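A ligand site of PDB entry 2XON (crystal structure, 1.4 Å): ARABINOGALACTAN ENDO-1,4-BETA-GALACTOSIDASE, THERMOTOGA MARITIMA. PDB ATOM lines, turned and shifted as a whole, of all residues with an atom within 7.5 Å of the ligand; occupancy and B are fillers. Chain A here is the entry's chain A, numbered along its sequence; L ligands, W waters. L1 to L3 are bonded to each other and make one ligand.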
ATOM      1  N   ALA A  32      29.471 -23.254 -15.107  1.00  0.00           N
ATOM      2  CA  ALA A  32      28.689 -22.625 -14.089  1.00  0.00           C
ATOM      3  C   ALA A  32      29.503 -21.674 -13.185  1.00  0.00           C
ATOM      4  O   ALA A  32      28.911 -21.029 -12.344  1.00  0.00           O
ATOM      5  CB  ALA A  32      27.922 -23.631 -13.188  1.00  0.00           C
ATOM      6  N   LYS A  34      32.899 -19.013 -12.381  1.00  0.00           N
ATOM      7  CA  LYS A  34      33.873 -18.054 -12.898  1.00  0.00           C
ATOM      8  C   LYS A  34      34.466 -17.297 -11.738  1.00  0.00           C
ATOM      9  O   LYS A  34      33.847 -17.155 -10.675  1.00  0.00           O
ATOM     10  CB  LYS A  34      33.216 -17.048 -13.840  1.00  0.00           C
ATOM     11  CG  LYS A  34      32.727 -17.605 -15.122  1.00  0.00           C
ATOM     12  CD  LYS A  34      31.966 -16.511 -15.860  1.00  0.00           C
ATOM     13  CE  LYS A  34      31.428 -16.980 -17.223  1.00  0.00           C
ATOM     14  NZ  LYS A  34      30.624 -15.873 -17.892  1.00  0.00           N
ATOM     15  N   VAL A  36      35.252 -13.486 -10.941  1.00  0.00           N
ATOM     16  CA  VAL A  36      34.825 -12.201 -11.474  1.00  0.00           C
ATOM     17  C   VAL A  36      35.302 -11.078 -10.554  1.00  0.00           C
ATOM     18  O   VAL A  36      35.478 -11.250  -9.350  1.00  0.00           O
ATOM     19  CB  VAL A  36      33.272 -12.118 -11.606  1.00  0.00           C
ATOM     20  CG1 VAL A  36      32.710 -13.302 -12.489  1.00  0.00           C
ATOM     21  CG2 VAL A  36      32.563 -12.122 -10.254  1.00  0.00           C
ATOM     22  N   ASN A  39      30.786  -6.765  -9.009  1.00  0.00           N
ATOM     23  CA  ASN A  39      30.095  -5.528  -9.317  1.00  0.00           C
ATOM     24  C   ASN A  39      28.597  -5.678  -8.950  1.00  0.00           C
ATOM     25  O   ASN A  39      27.870  -6.334  -9.696  1.00  0.00           O
ATOM     26  CB  ASN A  39      30.223  -5.103 -10.806  1.00  0.00           C
ATOM     27  CG  ASN A  39      29.504  -3.787 -11.097  1.00  0.00           C
ATOM     28  OD1 ASN A  39      28.891  -3.213 -10.228  1.00  0.00           O
ATOM     29  ND2 ASN A  39      29.569  -3.334 -12.357  1.00  0.00           N
ATOM     30  N   PRO A  40      28.161  -5.137  -7.806  1.00  0.00           N
ATOM     31  CA  PRO A  40      28.903  -4.281  -6.892  1.00  0.00           C
ATOM     32  C   PRO A  40      29.972  -5.055  -6.174  1.00  0.00           C
ATOM     33  O   PRO A  40      29.867  -6.288  -5.979  1.00  0.00           O
ATOM     34  CB  PRO A  40      27.810  -3.765  -5.955  1.00  0.00           C
ATOM     35  CG  PRO A  40      26.810  -4.850  -5.928  1.00  0.00           C
ATOM     36  CD  PRO A  40      26.785  -5.368  -7.318  1.00  0.00           C
ATOM     37  N   SER A  42      30.357  -5.267  -3.158  1.00  0.00           N
ATOM     38  CA  SER A  42      29.757  -5.948  -2.030  1.00  0.00           C
ATOM     39  C   SER A  42      29.503  -7.415  -2.265  1.00  0.00           C
ATOM     40  O   SER A  42      29.376  -8.169  -1.287  1.00  0.00           O
ATOM     41  CB  SER A  42      28.507  -5.221  -1.652  1.00  0.00           C
ATOM     42  OG  SER A  42      27.752  -5.125  -2.858  1.00  0.00           O
ATOM     43  N   ASN A  43      29.496  -7.889  -3.522  1.00  0.00           N
ATOM     44  CA  ASN A  43      29.358  -9.335  -3.768  1.00  0.00           C
ATOM     45  C   ASN A  43      30.583 -10.144  -3.334  1.00  0.00           C
ATOM     46  O   ASN A  43      30.442 -11.328  -3.089  1.00  0.00           O
ATOM     47  CB  ASN A  43      29.066  -9.627  -5.259  1.00  0.00           C
ATOM     48  CG  ASN A  43      27.643  -9.264  -5.611  1.00  0.00           C
ATOM     49  OD1 ASN A  43      26.752  -9.440  -4.754  1.00  0.00           O
ATOM     50  ND2 ASN A  43      27.407  -8.818  -6.855  1.00  0.00           N
ATOM     51  N   ASN A  52      31.947 -16.463  -8.739  1.00  0.00           N
ATOM     52  CA  ASN A  52      30.511 -16.324  -8.966  1.00  0.00           C
ATOM     53  C   ASN A  52      30.079 -17.523  -9.739  1.00  0.00           C
ATOM     54  O   ASN A  52      30.684 -17.903 -10.736  1.00  0.00           O
ATOM     55  CB  ASN A  52      30.291 -15.061  -9.833  1.00  0.00           C
ATOM     56  CG  ASN A  52      28.821 -14.653 -10.086  1.00  0.00           C
ATOM     57  OD1 ASN A  52      27.893 -14.965  -9.256  1.00  0.00           O
ATOM     58  ND2 ASN A  52      28.610 -13.932 -11.128  1.00  0.00           N
ATOM     59  N   PHE A  53      29.011 -18.161  -9.279  1.00  0.00           N
ATOM     60  CA  PHE A  53      28.418 -19.252 -10.014  1.00  0.00           C
ATOM     61  C   PHE A  53      27.002 -18.907 -10.412  1.00  0.00           C
ATOM     62  O   PHE A  53      26.309 -18.149  -9.731  1.00  0.00           O
ATOM     63  CB  PHE A  53      28.506 -20.552  -9.220  1.00  0.00           C
ATOM     64  CG  PHE A  53      27.795 -20.539  -7.852  1.00  0.00           C
ATOM     65  CD1 PHE A  53      26.454 -20.819  -7.765  1.00  0.00           C
ATOM     66  CD2 PHE A  53      28.484 -20.244  -6.655  1.00  0.00           C
ATOM     67  CE1 PHE A  53      25.793 -20.825  -6.552  1.00  0.00           C
ATOM     68  CE2 PHE A  53      27.805 -20.265  -5.461  1.00  0.00           C
ATOM     69  CZ  PHE A  53      26.459 -20.574  -5.415  1.00  0.00           C
ATOM     70  N   TRP A  54      26.616 -19.459 -11.541  1.00  0.00           N
ATOM     71  CA  TRP A  54      25.280 -19.250 -12.088  1.00  0.00           C
ATOM     72  C   TRP A  54      25.169 -20.105 -13.350  1.00  0.00           C
ATOM     73  O   TRP A  54      26.141 -20.261 -14.083  1.00  0.00           O
ATOM     74  CB  TRP A  54      25.092 -17.793 -12.519  1.00  0.00           C
ATOM     75  CG  TRP A  54      23.807 -17.578 -13.372  1.00  0.00           C
ATOM     76  CD1 TRP A  54      22.516 -17.421 -12.934  1.00  0.00           C
ATOM     77  CD2 TRP A  54      23.798 -17.504 -14.790  1.00  0.00           C
ATOM     78  NE1 TRP A  54      21.693 -17.291 -14.039  1.00  0.00           N
ATOM     79  CE2 TRP A  54      22.464 -17.248 -15.174  1.00  0.00           C
ATOM     80  CE3 TRP A  54      24.806 -17.479 -15.782  1.00  0.00           C
ATOM     81  CZ2 TRP A  54      22.094 -17.059 -16.522  1.00  0.00           C
ATOM     82  CZ3 TRP A  54      24.427 -17.296 -17.144  1.00  0.00           C
ATOM     83  CH2 TRP A  54      23.098 -17.062 -17.459  1.00  0.00           C
ATOM     84  N   LEU A  55      23.963 -20.615 -13.629  1.00  0.00           N
ATOM     85  CA  LEU A  55      23.714 -21.199 -14.949  1.00  0.00           C
ATOM     86  C   LEU A  55      22.264 -21.169 -15.158  1.00  0.00           C
ATOM     87  O   LEU A  55      21.486 -21.153 -14.221  1.00  0.00           O
ATOM     88  CB  LEU A  55      24.248 -22.627 -14.966  1.00  0.00           C
ATOM     89  CG  LEU A  55      24.538 -23.198 -16.311  1.00  0.00           C
ATOM     90  CD1 LEU A  55      25.773 -22.455 -17.002  1.00  0.00           C
ATOM     91  CD2 LEU A  55      24.693 -24.741 -16.222  1.00  0.00           C
ATOM     92  N   HIS A  81      27.313 -16.221  -0.241  1.00  0.00           N
ATOM     93  CA  HIS A  81      25.916 -15.775  -0.275  1.00  0.00           C
ATOM     94  C   HIS A  81      25.371 -16.117  -1.646  1.00  0.00           C
ATOM     95  O   HIS A  81      26.121 -16.350  -2.589  1.00  0.00           O
ATOM     96  CB  HIS A  81      25.714 -14.268   0.008  1.00  0.00           C
ATOM     97  CG  HIS A  81      26.334 -13.376  -1.022  1.00  0.00           C
ATOM     98  ND1 HIS A  81      25.614 -12.579  -1.890  1.00  0.00           N
ATOM     99  CD2 HIS A  81      27.651 -13.143  -1.267  1.00  0.00           C
ATOM    100  CE1 HIS A  81      26.490 -11.907  -2.660  1.00  0.00           C
ATOM    101  NE2 HIS A  81      27.720 -12.236  -2.299  1.00  0.00           N
ATOM    102  N   GLU A  83      21.403 -17.157  -4.069  1.00  0.00           N
ATOM    103  CA  GLU A  83      19.978 -17.389  -4.209  1.00  0.00           C
ATOM    104  C   GLU A  83      19.517 -18.341  -3.129  1.00  0.00           C
ATOM    105  O   GLU A  83      20.170 -19.319  -2.775  1.00  0.00           O
ATOM    106  CB  GLU A  83      19.752 -17.947  -5.581  1.00  0.00           C
ATOM    107  CG  GLU A  83      18.282 -18.241  -5.931  1.00  0.00           C
ATOM    108  CD  GLU A  83      17.394 -17.037  -6.037  1.00  0.00           C
ATOM    109  OE1 GLU A  83      17.811 -15.924  -6.102  1.00  0.00           O
ATOM    110  OE2 GLU A  83      16.156 -17.251  -6.078  1.00  0.00           O
ATOM    111  N   GLY A 108      19.571 -15.823   0.176  1.00  0.00           N
ATOM    112  CA  GLY A 108      19.329 -14.588  -0.490  1.00  0.00           C
ATOM    113  C   GLY A 108      20.558 -13.688  -0.616  1.00  0.00           C
ATOM    114  O   GLY A 108      21.593 -13.904   0.054  1.00  0.00           O
ATOM    115  N   TRP A 109      20.438 -12.679  -1.480  1.00  0.00           N
ATOM    116  CA  TRP A 109      21.580 -11.832  -1.810  1.00  0.00           C
ATOM    117  C   TRP A 109      22.133 -11.145  -0.583  1.00  0.00           C
ATOM    118  O   TRP A 109      21.409 -10.579   0.217  1.00  0.00           O
ATOM    119  CB  TRP A 109      21.069 -10.812  -2.812  1.00  0.00           C
ATOM    120  CG  TRP A 109      22.161  -9.923  -3.386  1.00  0.00           C
ATOM    121  CD1 TRP A 109      23.422 -10.285  -3.762  1.00  0.00           C
ATOM    122  CD2 TRP A 109      22.052  -8.523  -3.666  1.00  0.00           C
ATOM    123  NE1 TRP A 109      24.078  -9.175  -4.264  1.00  0.00           N
ATOM    124  CE2 TRP A 109      23.276  -8.092  -4.183  1.00  0.00           C
ATOM    125  CE3 TRP A 109      21.032  -7.562  -3.468  1.00  0.00           C
ATOM    126  CZ2 TRP A 109      23.502  -6.792  -4.545  1.00  0.00           C
ATOM    127  CZ3 TRP A 109      21.250  -6.294  -3.862  1.00  0.00           C
ATOM    128  CH2 TRP A 109      22.487  -5.911  -4.358  1.00  0.00           C
ATOM    129  N   LEU A 110      23.458 -11.266  -0.407  1.00  0.00           N
ATOM    130  CA  LEU A 110      24.175 -10.580   0.665  1.00  0.00           C
ATOM    131  C   LEU A 110      23.787 -11.060   2.047  1.00  0.00           C
ATOM    132  O   LEU A 110      24.126 -10.424   3.041  1.00  0.00           O
ATOM    133  CB  LEU A 110      24.128  -9.082   0.576  1.00  0.00           C
ATOM    134  CG  LEU A 110      24.631  -8.486  -0.715  1.00  0.00           C
ATOM    135  CD1 LEU A 110      24.413  -6.974  -0.764  1.00  0.00           C
ATOM    136  CD2 LEU A 110      26.151  -8.817  -0.939  1.00  0.00           C
ATOM    137  N   GLY A 138      18.971 -21.340 -12.921  1.00  0.00           N
ATOM    138  CA  GLY A 138      18.929 -19.970 -12.577  1.00  0.00           C
ATOM    139  C   GLY A 138      19.537 -19.578 -11.242  1.00  0.00           C
ATOM    140  O   GLY A 138      19.636 -18.381 -10.960  1.00  0.00           O
ATOM    141  N   ASP A 139      19.891 -20.571 -10.417  1.00  0.00           N
ATOM    142  CA  ASP A 139      20.495 -20.314  -9.122  1.00  0.00           C
ATOM    143  C   ASP A 139      21.890 -19.696  -9.334  1.00  0.00           C
ATOM    144  O   ASP A 139      22.505 -19.755 -10.395  1.00  0.00           O
ATOM    145  CB  ASP A 139      20.631 -21.554  -8.289  1.00  0.00           C
ATOM    146  CG  ASP A 139      19.327 -22.002  -7.635  1.00  0.00           C
ATOM    147  OD1 ASP A 139      18.341 -21.196  -7.729  1.00  0.00           O
ATOM    148  OD2 ASP A 139      19.368 -23.052  -7.013  1.00  0.00           O
ATOM    149  N   TRP A 140      22.357 -19.042  -8.306  1.00  0.00           N
ATOM    150  CA  TRP A 140      23.602 -18.226  -8.399  1.00  0.00           C
ATOM    151  C   TRP A 140      24.109 -18.014  -7.043  1.00  0.00           C
ATOM    152  O   TRP A 140      23.392 -18.081  -6.041  1.00  0.00           O
ATOM    153  CB  TRP A 140      23.319 -16.899  -9.123  1.00  0.00           C
ATOM    154  CG  TRP A 140      22.339 -16.065  -8.462  1.00  0.00           C
ATOM    155  CD1 TRP A 140      20.992 -16.103  -8.700  1.00  0.00           C
ATOM    156  CD2 TRP A 140      22.519 -15.141  -7.367  1.00  0.00           C
ATOM    157  NE1 TRP A 140      20.338 -15.287  -7.833  1.00  0.00           N
ATOM    158  CE2 TRP A 140      21.242 -14.667  -7.016  1.00  0.00           C
ATOM    159  CE3 TRP A 140      23.626 -14.614  -6.680  1.00  0.00           C
ATOM    160  CZ2 TRP A 140      21.053 -13.828  -5.953  1.00  0.00           C
ATOM    161  CZ3 TRP A 140      23.417 -13.718  -5.702  1.00  0.00           C
ATOM    162  CH2 TRP A 140      22.167 -13.337  -5.318  1.00  0.00           C
ATOM    163  N   GLY A 141      25.364 -17.567  -6.984  1.00  0.00           N
ATOM    164  CA  GLY A 141      25.948 -17.202  -5.695  1.00  0.00           C
ATOM    165  C   GLY A 141      27.390 -16.775  -5.866  1.00  0.00           C
ATOM    166  O   GLY A 141      27.932 -16.783  -6.950  1.00  0.00           O
ATOM    167  N   PHE A 142      27.983 -16.400  -4.720  1.00  0.00           N
ATOM    168  CA  PHE A 142      29.402 -15.959  -4.616  1.00  0.00           C
ATOM    169  C   PHE A 142      30.069 -16.720  -3.516  1.00  0.00           C
ATOM    170  O   PHE A 142      29.482 -16.979  -2.476  1.00  0.00           O
ATOM    171  CB  PHE A 142      29.511 -14.460  -4.404  1.00  0.00           C
ATOM    172  CG  PHE A 142      29.025 -13.607  -5.555  1.00  0.00           C
ATOM    173  CD1 PHE A 142      27.634 -13.305  -5.736  1.00  0.00           C
ATOM    174  CD2 PHE A 142      29.893 -13.146  -6.526  1.00  0.00           C
ATOM    175  CE1 PHE A 142      27.209 -12.533  -6.758  1.00  0.00           C
ATOM    176  CE2 PHE A 142      29.443 -12.373  -7.585  1.00  0.00           C
ATOM    177  CZ  PHE A 142      28.088 -12.047  -7.677  1.00  0.00           C
HETATM  178  C1  LIG L   1      25.388 -12.068 -17.634  1.00  0.00           C
HETATM  179  C2  LIG L   1      26.400 -12.667 -16.655  1.00  0.00           C
HETATM  180  C3  LIG L   1      25.831 -14.016 -16.235  1.00  0.00           C
HETATM  181  C4  LIG L   1      24.436 -13.885 -15.699  1.00  0.00           C
HETATM  182  C5  LIG L   1      23.530 -13.243 -16.728  1.00  0.00           C
HETATM  183  C6  LIG L   1      22.102 -13.004 -16.233  1.00  0.00           C
HETATM  184  O1  LIG L   1      25.714 -10.774 -18.093  1.00  0.00           O
HETATM  185  O2  LIG L   1      27.635 -12.752 -17.297  1.00  0.00           O
HETATM  186  O3  LIG L   1      26.659 -14.647 -15.273  1.00  0.00           O
HETATM  187  O4  LIG L   1      24.460 -13.102 -14.499  1.00  0.00           O
HETATM  188  O5  LIG L   1      24.068 -11.994 -17.088  1.00  0.00           O
HETATM  189  O6  LIG L   1      21.332 -12.665 -17.415  1.00  0.00           O
HETATM  190  C1  LG2 L   2      24.052 -13.717 -13.331  1.00  0.00           C
HETATM  191  C2  LG2 L   2      25.048 -13.383 -12.224  1.00  0.00           C
HETATM  192  C3  LG2 L   2      24.540 -13.914 -10.873  1.00  0.00           C
HETATM  193  C4  LG2 L   2      23.109 -13.399 -10.608  1.00  0.00           C
HETATM  194  C5  LG2 L   2      22.227 -13.803 -11.805  1.00  0.00           C
HETATM  195  C6  LG2 L   2      20.800 -13.276 -11.653  1.00  0.00           C
HETATM  196  O1  LG2 L   2      26.281 -14.042 -12.586  1.00  0.00           O
HETATM  197  O2  LG2 L   2      25.422 -13.524  -9.839  1.00  0.00           O
HETATM  198  O3  LG2 L   2      23.142 -12.010 -10.476  1.00  0.00           O
HETATM  199  O4  LG2 L   2      22.777 -13.240 -12.989  1.00  0.00           O
HETATM  200  O5  LG2 L   2      20.027 -13.820 -12.739  1.00  0.00           O
HETATM  201  C1  LG3 L   3      23.038 -11.484  -9.208  1.00  0.00           C
HETATM  202  C2  LG3 L   3      23.964 -10.288  -9.071  1.00  0.00           C
HETATM  203  C3  LG3 L   3      23.777  -9.578  -7.715  1.00  0.00           C
HETATM  204  C4  LG3 L   3      22.304  -9.258  -7.527  1.00  0.00           C
HETATM  205  C5  LG3 L   3      21.428 -10.517  -7.735  1.00  0.00           C
HETATM  206  C6  LG3 L   3      19.949 -10.265  -7.599  1.00  0.00           C
HETATM  207  O1  LG3 L   3      25.266 -10.852  -9.124  1.00  0.00           O
HETATM  208  O2  LG3 L   3      24.612  -8.430  -7.655  1.00  0.00           O
HETATM  209  O3  LG3 L   3      21.921  -8.250  -8.503  1.00  0.00           O
HETATM  210  O4  LG3 L   3      21.678 -11.130  -9.006  1.00  0.00           O
HETATM  211  O5  LG3 L   3      19.651  -9.803  -6.308  1.00  0.00           O
HETATM  212  O   HOH W   1      28.148 -16.694 -16.500  1.00  0.00           O
HETATM  213  O   HOH W   2      19.289 -14.163 -17.517  1.00  0.00           O
HETATM  214  O   HOH W   3      19.029 -16.339 -12.625  1.00  0.00           O
HETATM  215  O   HOH W   4      26.684  -9.141 -10.570  1.00  0.00           O
HETATM  216  O   HOH W   5      24.547  -6.537  -9.646  1.00  0.00           O
HETATM  217  O   HOH W   6      29.744 -13.491 -15.772  1.00  0.00           O
HETATM  218  O   HOH W   7      22.962 -10.145 -12.927  1.00  0.00           O
HETATM  219  O   HOH W   8      17.845 -11.466  -5.308  1.00  0.00           O
HETATM  220  O   HOH W   9      20.719  -9.913 -17.918  1.00  0.00           O
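Residues that only touch the ligand: Pro 40 (3.8 Å), Trp 54 (3.4 Å), Trp 109 (3.5 Å), Trp 140 (3.5 Å) and Phe 142 (3.4 Å). Hydrophobic or aromatic side chains that line the ligand: Pro 40, Trp 54, Trp 109, Trp 140 and Phe 142.
Water W4 lies within hydrogen-bond range of an oxygen (O1) of LG3 L3 and the backbone carbonyl oxygen (O) of Asn 39. Water W6 lies within hydrogen-bond range of O2 of LIG L1 (2.7 Å) and NZ of Lys 34 (3.3 Å). Water W3 lies within hydrogen-bond range of O of Gly 138 (2.7 Å), O5 of LG2 L2 (2.7 Å) and NE1 of Trp 54 (3.2 Å). Water W5 bridges O2 of LG3 L3 and O of Asn 39. Water W1 lies within hydrogen-bond range of an oxygen (O3) of LIG L1 (2.8 Å) and the side-chain amino group (NZ) of Lys 34 (3.0 Å).
The side-chain amide nitrogen (ND2) of Asn 52 lies within hydrogen-bond range of an oxygen (O1) of LG2 L2 (2.7 Å). An oxygen (O2) of LG3 L3 sits at hydrogen-bond distance from the side-chain amide nitrogen of Asn 43 (2.9 Å).
N of Asn 52 lies within hydrogen-bond range of O of Lys 34 (2.8 Å). The side-chain amide oxygen (OD1) of Asn 52 lies close to the backbone carbonyl oxygen (O) of Gly 141. The side-chain amide oxygen (OD1) of Asn 43 sits at hydrogen-bond distance from the indole nitrogen (NE1) of Trp 109 (2.7 Å). O of Asn 43 is in hydrogen-bond range of NE2 of His 81 (3.0 Å). N of Phe 142 is in hydrogen-bond range of O of His 81 (2.8 Å). The backbone carbonyl oxygen (O) of Ala 32 is in hydrogen-bond range of the backbone NH (N) of Trp 54 (2.9 Å). The backbone NH of Glu 83 sits at hydrogen-bond distance from the backbone carbonyl oxygen of Trp 140, at 2.9 Å.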
